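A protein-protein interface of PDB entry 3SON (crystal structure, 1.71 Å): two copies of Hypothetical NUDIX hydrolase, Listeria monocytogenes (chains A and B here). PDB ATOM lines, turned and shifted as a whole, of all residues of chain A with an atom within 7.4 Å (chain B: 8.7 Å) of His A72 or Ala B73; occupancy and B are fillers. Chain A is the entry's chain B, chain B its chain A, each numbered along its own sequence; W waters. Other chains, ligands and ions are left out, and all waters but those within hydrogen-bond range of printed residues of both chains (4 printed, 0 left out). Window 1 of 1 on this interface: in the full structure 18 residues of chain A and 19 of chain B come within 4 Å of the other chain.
Hydrophobic or aromatic side chains of chain A that line the printed part of chain B: His A72.
O of Ser A71 lies within hydrogen-bond range of SG of Cys A92. The backbone carbonyl oxygen of Ala B73 is in hydrogen-bond range of the backbone NH of Glu B90. The backbone NH of Asp A70 lies within hydrogen-bond range of the side-chain carboxylate of Glu A136 (2.8 Å). The side-chain hydroxyl (OG) of Ser A71 sits at hydrogen-bond distance from the side-chain carboxylate (OE1) of Glu A136. The backbone carbonyl oxygen (O) of Asp A70 is in hydrogen-bond range of a ring nitrogen (ND1) of His A72, at 3.0 Å. O of Ser B71 lies within hydrogen-bond range of SG of Cys B92 (3.3 Å).
CG2 of Val B87 touches CB of Asp A70, at 3.8 Å. Ser A71 touches Ser B74 (CA to OG, 3.5 Å). Val B87 touches Ser A71 (CG1 to OG, 3.5 Å). NE2 of His A72 touches CE1 of His B72, at 3.1 Å. His A72 touches Ala B73. Ser A74 touches Asp B70. Thr B132 touches Ser A74 (CG2 to O, 3.7 Å). Ser B74 touches Thr A132 (O to CG2, 3.5 Å). CG2 of Thr A132 touches CG1 of Val B87 (3.9 Å). Glu A136 touches Val B87 (OE1 to CG2, 3.9 Å).
Ser A71 touches Ser B74, and with the chains exchanged Ser A74 touches Ser B71. His A72 touches Ala B73, and with the chains exchanged Ala A73 touches His B72. Ser A74 touches Asp B70, but with the chains exchanged Asp A70 does not touch Ser B74 (4.02 Å). Ser A74 touches Thr B132, and with the chains exchanged Thr A132 touches Ser B74.
The backbone NH (N) of His B72 is in hydrogen-bond range of the side-chain hydroxyl (OG) of Ser A74. OG of Ser B74 is in hydrogen-bond range of N of His A72.
Water W1 bridges O of Ser A74 (2.5 Å) and OG1 of Thr B132 (2.7 Å). Water W2 lies within hydrogen-bond range of N of Ser A129 and OD2 of Asp B128. Water W4 bridges the backbone NH of Ser B74 (3.1 Å) and the backbone carbonyl oxygen of His A72 (3.4 Å). Water W3 lies within hydrogen-bond range of O of His B72 (3.2 Å) and N of Ser A74 (3.3 Å).
Ser A71 touches two residues of chain B. Of the printed residues of chain B, His A72 touches His B72, Ala B73 and Ser B74. Of the printed residues of chain B, Thr A132 touches Ser B74 (3.5 Å), Pro B76 (3.6 Å) and Val B87 (3.9 Å). Of the printed residues of chain A, His B72 touches His A72 (3.1 Å), Ala A73 (3.3 Å) and Ser A74 (2.9 Å). Of the printed residues of chain A, Ala B73 touches His A72. Phe B80 touches none of the printed residues of chain A. The nearest residue of chain A that does not touch Ala B73 is Ala A73 (4.2 Å).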
ATOM      1  N   LEU A  69      11.895 -22.259 -32.084  1.00  0.00           N
ATOM      2  CA  LEU A  69      12.569 -21.150 -32.814  1.00  0.00           C
ATOM      3  C   LEU A  69      14.084 -21.323 -32.641  1.00  0.00           C
ATOM      4  O   LEU A  69      14.490 -21.961 -31.693  1.00  0.00           O
ATOM      5  CB  LEU A  69      12.148 -19.780 -32.285  1.00  0.00           C
ATOM      6  CG  LEU A  69      10.673 -19.388 -32.502  1.00  0.00           C
ATOM      7  CD1 LEU A  69      10.257 -18.201 -31.639  1.00  0.00           C
ATOM      8  CD2 LEU A  69      10.286 -19.115 -33.966  1.00  0.00           C
ATOM      9  N   ASP A  70      14.872 -20.887 -33.641  1.00  0.00           N
ATOM     10  CA  ASP A  70      16.351 -20.907 -33.543  1.00  0.00           C
ATOM     11  C   ASP A  70      16.910 -19.991 -32.455  1.00  0.00           C
ATOM     12  O   ASP A  70      17.947 -20.266 -31.841  1.00  0.00           O
ATOM     13  CB  ASP A  70      16.991 -20.454 -34.839  1.00  0.00           C
ATOM     14  CG  ASP A  70      16.778 -21.393 -35.948  1.00  0.00           C
ATOM     15  OD1 ASP A  70      16.798 -22.607 -35.699  1.00  0.00           O
ATOM     16  OD2 ASP A  70      16.610 -20.892 -37.077  1.00  0.00           O
ATOM     17  N   SER A  71      16.229 -18.880 -32.219  1.00  0.00           N
ATOM     18  CA  SER A  71      16.737 -17.857 -31.295  1.00  0.00           C
ATOM     19  C   SER A  71      16.967 -18.391 -29.893  1.00  0.00           C
ATOM     20  O   SER A  71      16.139 -19.095 -29.345  1.00  0.00           O
ATOM     21  CB  SER A  71      15.791 -16.620 -31.238  1.00  0.00           C
ATOM     22  OG  SER A  71      15.736 -15.964 -32.488  1.00  0.00           O
ATOM     23  N   HIS A  72      18.161 -18.140 -29.368  1.00  0.00           N
ATOM     24  CA  HIS A  72      18.423 -18.404 -27.968  1.00  0.00           C
ATOM     25  C   HIS A  72      19.451 -17.503 -27.440  1.00  0.00           C
ATOM     26  O   HIS A  72      20.190 -16.873 -28.201  1.00  0.00           O
ATOM     27  CB  HIS A  72      18.757 -19.895 -27.747  1.00  0.00           C
ATOM     28  CG  HIS A  72      20.003 -20.359 -28.414  1.00  0.00           C
ATOM     29  ND1 HIS A  72      20.095 -20.538 -29.761  1.00  0.00           N
ATOM     30  CD2 HIS A  72      21.208 -20.768 -27.879  1.00  0.00           C
ATOM     31  CE1 HIS A  72      21.308 -21.018 -30.055  1.00  0.00           C
ATOM     32  NE2 HIS A  72      21.984 -21.178 -28.905  1.00  0.00           N
ATOM     33  N   ALA A  73      19.480 -17.364 -26.139  1.00  0.00           N
ATOM     34  CA  ALA A  73      20.373 -16.432 -25.547  1.00  0.00           C
ATOM     35  C   ALA A  73      20.713 -16.864 -24.157  1.00  0.00           C
ATOM     36  O   ALA A  73      19.984 -17.619 -23.522  1.00  0.00           O
ATOM     37  CB  ALA A  73      19.719 -15.073 -25.489  1.00  0.00           C
ATOM     38  N   SER A  74      21.752 -16.279 -23.637  1.00  0.00           N
ATOM     39  CA  SER A  74      22.160 -16.574 -22.259  1.00  0.00           C
ATOM     40  C   SER A  74      21.586 -15.564 -21.266  1.00  0.00           C
ATOM     41  O   SER A  74      21.354 -14.387 -21.603  1.00  0.00           O
ATOM     42  CB  SER A  74      23.694 -16.664 -22.152  1.00  0.00           C
ATOM     43  OG  SER A  74      24.339 -17.539 -23.112  1.00  0.00           O
ATOM     44  N   PRO A  89      21.155 -20.987 -20.626  1.00  0.00           N
ATOM     45  CA  PRO A  89      20.554 -20.750 -21.892  1.00  0.00           C
ATOM     46  C   PRO A  89      19.058 -20.579 -21.800  1.00  0.00           C
ATOM     47  O   PRO A  89      18.356 -21.178 -20.934  1.00  0.00           O
ATOM     48  CB  PRO A  89      20.901 -22.033 -22.653  1.00  0.00           C
ATOM     49  CG  PRO A  89      20.859 -23.080 -21.560  1.00  0.00           C
ATOM     50  CD  PRO A  89      21.555 -22.411 -20.450  1.00  0.00           C
ATOM     51  N   GLU A  90      18.563 -19.722 -22.662  1.00  0.00           N
ATOM     52  CA  GLU A  90      17.117 -19.492 -22.767  1.00  0.00           C
ATOM     53  C   GLU A  90      16.674 -19.947 -24.139  1.00  0.00           C
ATOM     54  O   GLU A  90      17.056 -19.300 -25.143  1.00  0.00           O
ATOM     55  CB  GLU A  90      16.783 -17.998 -22.553  1.00  0.00           C
ATOM     56  CG  GLU A  90      15.293 -17.692 -22.680  1.00  0.00           C
ATOM     57  CD  GLU A  90      15.002 -16.171 -22.735  1.00  0.00           C
ATOM     58  OE1 GLU A  90      15.604 -15.462 -23.608  1.00  0.00           O
ATOM     59  OE2 GLU A  90      14.226 -15.717 -21.876  1.00  0.00           O
ATOM     60  N   TYR A  91      15.849 -21.010 -24.191  1.00  0.00           N
ATOM     61  CA  TYR A  91      15.403 -21.607 -25.438  1.00  0.00           C
ATOM     62  C   TYR A  91      13.987 -21.122 -25.779  1.00  0.00           C
ATOM     63  O   TYR A  91      13.142 -21.076 -24.909  1.00  0.00           O
ATOM     64  CB  TYR A  91      15.472 -23.176 -25.317  1.00  0.00           C
ATOM     65  CG  TYR A  91      16.919 -23.701 -25.067  1.00  0.00           C
ATOM     66  CD1 TYR A  91      17.919 -23.567 -26.036  1.00  0.00           C
ATOM     67  CD2 TYR A  91      17.280 -24.286 -23.873  1.00  0.00           C
ATOM     68  CE1 TYR A  91      19.223 -23.987 -25.795  1.00  0.00           C
ATOM     69  CE2 TYR A  91      18.559 -24.707 -23.631  1.00  0.00           C
ATOM     70  CZ  TYR A  91      19.521 -24.607 -24.596  1.00  0.00           C
ATOM     71  OH  TYR A  91      20.810 -25.021 -24.327  1.00  0.00           O
ATOM     72  N   CYS A  92      13.744 -20.794 -27.064  1.00  0.00           N
ATOM     73  CA  CYS A  92      12.523 -20.125 -27.470  1.00  0.00           C
ATOM     74  C   CYS A  92      11.568 -20.974 -28.338  1.00  0.00           C
ATOM     75  O   CYS A  92      12.009 -21.824 -29.120  1.00  0.00           O
ATOM     76  CB  CYS A  92      12.862 -18.837 -28.259  1.00  0.00           C
ATOM     77  SG  CYS A  92      13.904 -17.696 -27.316  1.00  0.00           S
ATOM     78  N   SER A 129      16.387 -10.388 -25.939  1.00  0.00           N
ATOM     79  CA  SER A 129      16.181 -11.795 -26.337  1.00  0.00           C
ATOM     80  C   SER A 129      14.754 -12.078 -26.833  1.00  0.00           C
ATOM     81  O   SER A 129      14.566 -12.887 -27.718  1.00  0.00           O
ATOM     82  CB  SER A 129      16.577 -12.749 -25.208  1.00  0.00           C
ATOM     83  OG  SER A 129      15.651 -12.778 -24.166  1.00  0.00           O
ATOM     84  N   THR A 132      14.378 -10.429 -30.329  1.00  0.00           N
ATOM     85  CA  THR A 132      15.022 -11.225 -31.409  1.00  0.00           C
ATOM     86  C   THR A 132      14.130 -12.442 -31.754  1.00  0.00           C
ATOM     87  O   THR A 132      13.811 -12.685 -32.903  1.00  0.00           O
ATOM     88  CB  THR A 132      16.442 -11.699 -30.985  1.00  0.00           C
ATOM     89  OG1 THR A 132      17.262 -10.528 -30.817  1.00  0.00           O
ATOM     90  CG2 THR A 132      17.084 -12.590 -32.089  1.00  0.00           C
ATOM     91  N   ALA A 133      13.696 -13.162 -30.730  1.00  0.00           N
ATOM     92  CA  ALA A 133      12.813 -14.322 -30.864  1.00  0.00           C
ATOM     93  C   ALA A 133      11.525 -13.929 -31.642  1.00  0.00           C
ATOM     94  O   ALA A 133      11.084 -14.630 -32.526  1.00  0.00           O
ATOM     95  CB  ALA A 133      12.449 -14.860 -29.465  1.00  0.00           C
ATOM     96  N   GLU A 136      12.247 -13.314 -35.390  1.00  0.00           N
ATOM     97  CA  GLU A 136      12.343 -14.621 -36.092  1.00  0.00           C
ATOM     98  C   GLU A 136      10.932 -15.196 -36.342  1.00  0.00           C
ATOM     99  O   GLU A 136      10.608 -15.579 -37.471  1.00  0.00           O
ATOM    100  CB  GLU A 136      13.153 -15.623 -35.262  1.00  0.00           C
ATOM    101  CG  GLU A 136      13.327 -16.940 -35.970  1.00  0.00           C
ATOM    102  CD  GLU A 136      13.928 -18.020 -35.135  1.00  0.00           C
ATOM    103  OE1 GLU A 136      14.447 -17.725 -34.017  1.00  0.00           O
ATOM    104  OE2 GLU A 136      13.872 -19.193 -35.613  1.00  0.00           O
ATOM    105  N   PHE B   6      28.007 -16.226 -38.788  1.00  0.00           N
ATOM    106  CA  PHE B   6      27.993 -16.013 -37.355  1.00  0.00           C
ATOM    107  C   PHE B   6      28.727 -14.754 -37.089  1.00  0.00           C
ATOM    108  O   PHE B   6      29.454 -14.279 -37.954  1.00  0.00           O
ATOM    109  CB  PHE B   6      28.702 -17.173 -36.630  1.00  0.00           C
ATOM    110  CG  PHE B   6      30.193 -17.333 -37.010  1.00  0.00           C
ATOM    111  CD1 PHE B   6      31.178 -16.584 -36.360  1.00  0.00           C
ATOM    112  CD2 PHE B   6      30.580 -18.241 -37.964  1.00  0.00           C
ATOM    113  CE1 PHE B   6      32.529 -16.723 -36.668  1.00  0.00           C
ATOM    114  CE2 PHE B   6      31.934 -18.409 -38.302  1.00  0.00           C
ATOM    115  CZ  PHE B   6      32.905 -17.632 -37.661  1.00  0.00           C
ATOM    116  N   GLN B   7      28.643 -14.281 -35.843  1.00  0.00           N
ATOM    117  CA  GLN B   7      29.290 -13.100 -35.366  1.00  0.00           C
ATOM    118  C   GLN B   7      30.136 -13.410 -34.133  1.00  0.00           C
ATOM    119  O   GLN B   7      29.895 -14.398 -33.423  1.00  0.00           O
ATOM    120  CB  GLN B   7      28.242 -12.089 -34.908  1.00  0.00           C
ATOM    121  CG  GLN B   7      27.545 -11.351 -36.037  1.00  0.00           C
ATOM    122  CD  GLN B   7      28.392 -10.263 -36.607  1.00  0.00           C
ATOM    123  OE1 GLN B   7      28.892  -9.382 -35.892  1.00  0.00           O
ATOM    124  NE2 GLN B   7      28.607 -10.329 -37.875  1.00  0.00           N
ATOM    125  N   VAL B   8      31.147 -12.616 -33.927  1.00  0.00           N
ATOM    126  CA  VAL B   8      31.880 -12.693 -32.709  1.00  0.00           C
ATOM    127  C   VAL B   8      31.834 -11.371 -31.948  1.00  0.00           C
ATOM    128  O   VAL B   8      31.626 -10.262 -32.551  1.00  0.00           O
ATOM    129  CB  VAL B   8      33.336 -13.233 -32.897  1.00  0.00           C
ATOM    130  CG1 VAL B   8      33.393 -14.577 -33.700  1.00  0.00           C
ATOM    131  CG2 VAL B   8      34.232 -12.189 -33.607  1.00  0.00           C
ATOM    132  N   LEU B   9      31.931 -11.488 -30.626  1.00  0.00           N
ATOM    133  CA  LEU B   9      32.077 -10.354 -29.734  1.00  0.00           C
ATOM    134  C   LEU B   9      33.356 -10.612 -28.945  1.00  0.00           C
ATOM    135  O   LEU B   9      33.641 -11.751 -28.547  1.00  0.00           O
ATOM    136  CB  LEU B   9      30.874 -10.193 -28.799  1.00  0.00           C
ATOM    137  CG  LEU B   9      30.836  -8.962 -27.886  1.00  0.00           C
ATOM    138  CD1 LEU B   9      30.168  -7.807 -28.611  1.00  0.00           C
ATOM    139  CD2 LEU B   9      30.085  -9.299 -26.600  1.00  0.00           C
ATOM    140  N   ASP B  70      31.011 -18.534 -22.280  1.00  0.00           N
ATOM    141  CA  ASP B  70      29.757 -19.281 -22.562  1.00  0.00           C
ATOM    142  C   ASP B  70      28.600 -18.413 -23.055  1.00  0.00           C
ATOM    143  O   ASP B  70      27.693 -18.912 -23.689  1.00  0.00           O
ATOM    144  CB  ASP B  70      29.279 -20.037 -21.315  1.00  0.00           C
ATOM    145  CG  ASP B  70      30.215 -21.102 -20.878  1.00  0.00           C
ATOM    146  OD1 ASP B  70      30.631 -21.904 -21.749  1.00  0.00           O
ATOM    147  OD2 ASP B  70      30.500 -21.163 -19.647  1.00  0.00           O
ATOM    148  N   SER B  71      28.624 -17.129 -22.781  1.00  0.00           N
ATOM    149  CA  SER B  71      27.504 -16.291 -23.161  1.00  0.00           C
ATOM    150  C   SER B  71      27.348 -16.265 -24.667  1.00  0.00           C
ATOM    151  O   SER B  71      28.302 -16.067 -25.386  1.00  0.00           O
ATOM    152  CB  SER B  71      27.647 -14.850 -22.589  1.00  0.00           C
ATOM    153  OG  SER B  71      27.578 -14.810 -21.193  1.00  0.00           O
ATOM    154  N   HIS B  72      26.140 -16.517 -25.125  1.00  0.00           N
ATOM    155  CA  HIS B  72      25.836 -16.532 -26.529  1.00  0.00           C
ATOM    156  C   HIS B  72      24.478 -15.924 -26.765  1.00  0.00           C
ATOM    157  O   HIS B  72      23.585 -16.070 -25.929  1.00  0.00           O
ATOM    158  CB  HIS B  72      25.924 -18.012 -27.007  1.00  0.00           C
ATOM    159  CG  HIS B  72      25.107 -18.316 -28.222  1.00  0.00           C
ATOM    160  ND1 HIS B  72      23.768 -18.170 -28.241  1.00  0.00           N
ATOM    161  CD2 HIS B  72      25.475 -18.780 -29.485  1.00  0.00           C
ATOM    162  CE1 HIS B  72      23.297 -18.478 -29.464  1.00  0.00           C
ATOM    163  NE2 HIS B  72      24.342 -18.883 -30.221  1.00  0.00           N
ATOM    164  N   ALA B  73      24.292 -15.246 -27.901  1.00  0.00           N
ATOM    165  CA  ALA B  73      22.990 -14.670 -28.286  1.00  0.00           C
ATOM    166  C   ALA B  73      22.711 -14.745 -29.800  1.00  0.00           C
ATOM    167  O   ALA B  73      23.588 -14.874 -30.583  1.00  0.00           O
ATOM    168  CB  ALA B  73      22.880 -13.211 -27.839  1.00  0.00           C
ATOM    169  N   SER B  74      21.447 -14.730 -30.172  1.00  0.00           N
ATOM    170  CA  SER B  74      21.092 -14.717 -31.576  1.00  0.00           C
ATOM    171  C   SER B  74      20.889 -13.279 -31.959  1.00  0.00           C
ATOM    172  O   SER B  74      20.481 -12.458 -31.129  1.00  0.00           O
ATOM    173  CB  SER B  74      19.838 -15.579 -31.797  1.00  0.00           C
ATOM    174  OG  SER B  74      20.095 -16.903 -31.389  1.00  0.00           O
ATOM    175  N   ILE B  75      21.216 -12.913 -33.175  1.00  0.00           N
ATOM    176  CA  ILE B  75      20.963 -11.558 -33.652  1.00  0.00           C
ATOM    177  C   ILE B  75      20.192 -11.623 -34.942  1.00  0.00           C
ATOM    178  O   ILE B  75      20.497 -12.467 -35.780  1.00  0.00           O
ATOM    179  CB  ILE B  75      22.285 -10.802 -33.942  1.00  0.00           C
ATOM    180  CG1 ILE B  75      23.210 -10.776 -32.744  1.00  0.00           C
ATOM    181  CG2 ILE B  75      22.010  -9.362 -34.356  1.00  0.00           C
ATOM    182  CD1 ILE B  75      24.590 -10.241 -33.128  1.00  0.00           C
ATOM    183  N   PRO B  76      19.189 -10.720 -35.132  1.00  0.00           N
ATOM    184  CA  PRO B  76      18.466 -10.624 -36.424  1.00  0.00           C
ATOM    185  C   PRO B  76      19.533 -10.492 -37.485  1.00  0.00           C
ATOM    186  O   PRO B  76      20.419  -9.628 -37.397  1.00  0.00           O
ATOM    187  CB  PRO B  76      17.610  -9.374 -36.252  1.00  0.00           C
ATOM    188  CG  PRO B  76      17.367  -9.311 -34.769  1.00  0.00           C
ATOM    189  CD  PRO B  76      18.601  -9.842 -34.103  1.00  0.00           C
ATOM    190  N   PHE B  80      23.382  -7.795 -40.626  1.00  0.00           N
ATOM    191  CA  PHE B  80      24.679  -8.342 -41.175  1.00  0.00           C
ATOM    192  C   PHE B  80      24.594  -8.898 -42.576  1.00  0.00           C
ATOM    193  O   PHE B  80      25.583  -8.848 -43.353  1.00  0.00           O
ATOM    194  CB  PHE B  80      25.193  -9.492 -40.263  1.00  0.00           C
ATOM    195  CG  PHE B  80      25.170  -9.178 -38.806  1.00  0.00           C
ATOM    196  CD1 PHE B  80      25.912  -8.122 -38.305  1.00  0.00           C
ATOM    197  CD2 PHE B  80      24.433  -9.976 -37.902  1.00  0.00           C
ATOM    198  CE1 PHE B  80      25.891  -7.820 -36.955  1.00  0.00           C
ATOM    199  CE2 PHE B  80      24.411  -9.683 -36.559  1.00  0.00           C
ATOM    200  CZ  PHE B  80      25.127  -8.574 -36.084  1.00  0.00           C
ATOM    201  N   VAL B  87      18.131 -15.511 -38.011  1.00  0.00           N
ATOM    202  CA  VAL B  87      18.979 -15.032 -36.909  1.00  0.00           C
ATOM    203  C   VAL B  87      20.331 -15.742 -36.947  1.00  0.00           C
ATOM    204  O   VAL B  87      20.422 -16.873 -37.461  1.00  0.00           O
ATOM    205  CB  VAL B  87      18.296 -15.267 -35.552  1.00  0.00           C
ATOM    206  CG1 VAL B  87      16.964 -14.527 -35.479  1.00  0.00           C
ATOM    207  CG2 VAL B  87      18.022 -16.791 -35.312  1.00  0.00           C
ATOM    208  N   VAL B  88      21.407 -15.110 -36.467  1.00  0.00           N
ATOM    209  CA  VAL B  88      22.730 -15.793 -36.422  1.00  0.00           C
ATOM    210  C   VAL B  88      23.297 -15.743 -35.042  1.00  0.00           C
ATOM    211  O   VAL B  88      22.932 -14.844 -34.216  1.00  0.00           O
ATOM    212  CB  VAL B  88      23.787 -15.182 -37.378  1.00  0.00           C
ATOM    213  CG1 VAL B  88      23.499 -15.559 -38.821  1.00  0.00           C
ATOM    214  CG2 VAL B  88      23.901 -13.681 -37.186  1.00  0.00           C
ATOM    215  N   PRO B  89      24.172 -16.693 -34.715  1.00  0.00           N
ATOM    216  CA  PRO B  89      24.668 -16.658 -33.383  1.00  0.00           C
ATOM    217  C   PRO B  89      25.805 -15.672 -33.231  1.00  0.00           C
ATOM    218  O   PRO B  89      26.555 -15.434 -34.171  1.00  0.00           O
ATOM    219  CB  PRO B  89      25.206 -18.089 -33.177  1.00  0.00           C
ATOM    220  CG  PRO B  89      25.624 -18.494 -34.505  1.00  0.00           C
ATOM    221  CD  PRO B  89      24.623 -17.922 -35.440  1.00  0.00           C
ATOM    222  N   GLU B  90      25.905 -15.133 -32.041  1.00  0.00           N
ATOM    223  CA  GLU B  90      27.007 -14.296 -31.626  1.00  0.00           C
ATOM    224  C   GLU B  90      27.795 -14.988 -30.480  1.00  0.00           C
ATOM    225  O   GLU B  90      27.264 -15.210 -29.365  1.00  0.00           O
ATOM    226  CB  GLU B  90      26.474 -12.949 -31.133  1.00  0.00           C
ATOM    227  CG  GLU B  90      27.545 -11.990 -30.759  1.00  0.00           C
ATOM    228  CD  GLU B  90      27.014 -10.713 -30.141  1.00  0.00           C
ATOM    229  OE1 GLU B  90      26.319 -10.778 -29.080  1.00  0.00           O
ATOM    230  OE2 GLU B  90      27.290  -9.646 -30.726  1.00  0.00           O
ATOM    231  N   TYR B  91      29.045 -15.320 -30.741  1.00  0.00           N
ATOM    232  CA  TYR B  91      29.909 -15.996 -29.788  1.00  0.00           C
ATOM    233  C   TYR B  91      30.802 -14.980 -29.152  1.00  0.00           C
ATOM    234  O   TYR B  91      31.243 -14.091 -29.807  1.00  0.00           O
ATOM    235  CB  TYR B  91      30.770 -17.023 -30.513  1.00  0.00           C
ATOM    236  CG  TYR B  91      29.972 -18.078 -31.269  1.00  0.00           C
ATOM    237  CD1 TYR B  91      29.380 -19.114 -30.583  1.00  0.00           C
ATOM    238  CD2 TYR B  91      29.776 -17.999 -32.649  1.00  0.00           C
ATOM    239  CE1 TYR B  91      28.645 -20.068 -31.242  1.00  0.00           C
ATOM    240  CE2 TYR B  91      29.047 -18.964 -33.340  1.00  0.00           C
ATOM    241  CZ  TYR B  91      28.479 -19.998 -32.608  1.00  0.00           C
ATOM    242  OH  TYR B  91      27.761 -20.987 -33.203  1.00  0.00           O
ATOM    243  N   CYS B  92      31.126 -15.161 -27.868  1.00  0.00           N
ATOM    244  CA  CYS B  92      31.779 -14.160 -27.155  1.00  0.00           C
ATOM    245  C   CYS B  92      33.133 -14.551 -26.623  1.00  0.00           C
ATOM    246  O   CYS B  92      33.358 -15.746 -26.194  1.00  0.00           O
ATOM    247  CB  CYS B  92      30.928 -13.728 -25.966  1.00  0.00           C
ATOM    248  SG  CYS B  92      29.319 -13.068 -26.394  1.00  0.00           S
ATOM    249  N   TRP B 127      23.180  -3.334 -25.367  1.00  0.00           N
ATOM    250  CA  TRP B 127      22.508  -4.615 -25.635  1.00  0.00           C
ATOM    251  C   TRP B 127      22.631  -5.607 -24.498  1.00  0.00           C
ATOM    252  O   TRP B 127      23.688  -5.754 -23.856  1.00  0.00           O
ATOM    253  CB  TRP B 127      23.039  -5.250 -26.897  1.00  0.00           C
ATOM    254  CG  TRP B 127      23.048  -4.342 -28.098  1.00  0.00           C
ATOM    255  CD1 TRP B 127      24.155  -3.950 -28.843  1.00  0.00           C
ATOM    256  CD2 TRP B 127      21.906  -3.689 -28.710  1.00  0.00           C
ATOM    257  NE1 TRP B 127      23.761  -3.109 -29.886  1.00  0.00           N
ATOM    258  CE2 TRP B 127      22.428  -2.898 -29.828  1.00  0.00           C
ATOM    259  CE3 TRP B 127      20.537  -3.635 -28.420  1.00  0.00           C
ATOM    260  CZ2 TRP B 127      21.600  -2.112 -30.623  1.00  0.00           C
ATOM    261  CZ3 TRP B 127      19.711  -2.844 -29.227  1.00  0.00           C
ATOM    262  CH2 TRP B 127      20.234  -2.101 -30.306  1.00  0.00           C
ATOM    263  N   ASP B 128      21.520  -6.231 -24.166  1.00  0.00           N
ATOM    264  CA  ASP B 128      21.511  -7.207 -23.080  1.00  0.00           C
ATOM    265  C   ASP B 128      22.622  -8.216 -23.312  1.00  0.00           C
ATOM    266  O   ASP B 128      23.342  -8.622 -22.356  1.00  0.00           O
ATOM    267  CB  ASP B 128      20.146  -7.910 -23.032  1.00  0.00           C
ATOM    268  CG  ASP B 128      18.969  -6.953 -22.667  1.00  0.00           C
ATOM    269  OD1 ASP B 128      19.243  -5.874 -22.138  1.00  0.00           O
ATOM    270  OD2 ASP B 128      17.770  -7.304 -22.918  1.00  0.00           O
ATOM    271  N   SER B 129      22.770  -8.675 -24.544  1.00  0.00           N
ATOM    272  CA  SER B 129      23.787  -9.681 -24.892  1.00  0.00           C
ATOM    273  C   SER B 129      25.240  -9.327 -24.440  1.00  0.00           C
ATOM    274  O   SER B 129      26.007 -10.148 -23.914  1.00  0.00           O
ATOM    275  CB  SER B 129      23.740 -10.004 -26.392  1.00  0.00           C
ATOM    276  OG  SER B 129      24.445  -9.063 -27.191  1.00  0.00           O
ATOM    277  N   ASN B 130      25.614  -8.084 -24.629  1.00  0.00           N
ATOM    278  CA  ASN B 130      26.912  -7.584 -24.186  1.00  0.00           C
ATOM    279  C   ASN B 130      27.090  -7.455 -22.654  1.00  0.00           C
ATOM    280  O   ASN B 130      28.146  -7.840 -22.108  1.00  0.00           O
ATOM    281  CB  ASN B 130      27.137  -6.212 -24.788  1.00  0.00           C
ATOM    282  CG  ASN B 130      27.098  -6.189 -26.296  1.00  0.00           C
ATOM    283  OD1 ASN B 130      26.790  -7.204 -27.022  1.00  0.00           O
ATOM    284  ND2 ASN B 130      27.383  -4.999 -26.809  1.00  0.00           N
ATOM    285  N   THR B 132      25.415  -9.295 -20.563  1.00  0.00           N
ATOM    286  CA  THR B 132      25.466 -10.668 -20.092  1.00  0.00           C
ATOM    287  C   THR B 132      26.871 -11.254 -20.229  1.00  0.00           C
ATOM    288  O   THR B 132      27.390 -11.826 -19.246  1.00  0.00           O
ATOM    289  CB  THR B 132      24.439 -11.555 -20.769  1.00  0.00           C
ATOM    290  OG1 THR B 132      23.131 -11.069 -20.416  1.00  0.00           O
ATOM    291  CG2 THR B 132      24.588 -13.061 -20.309  1.00  0.00           C
ATOM    292  N   ALA B 133      27.492 -11.097 -21.395  1.00  0.00           N
ATOM    293  CA  ALA B 133      28.897 -11.516 -21.608  1.00  0.00           C
ATOM    294  C   ALA B 133      29.879 -10.847 -20.591  1.00  0.00           C
ATOM    295  O   ALA B 133      30.795 -11.514 -19.959  1.00  0.00           O
ATOM    296  CB  ALA B 133      29.320 -11.269 -23.087  1.00  0.00           C
HETATM  297  O   HOH W   1      21.682 -12.044 -22.461  1.00  0.00           O
HETATM  298  O   HOH W   2      17.638 -10.235 -23.294  1.00  0.00           O
HETATM  299  O   HOH W   3      23.450 -13.529 -24.050  1.00  0.00           O
HETATM  300  O   HOH W   4      18.847 -13.859 -28.789  1.00  0.00           O
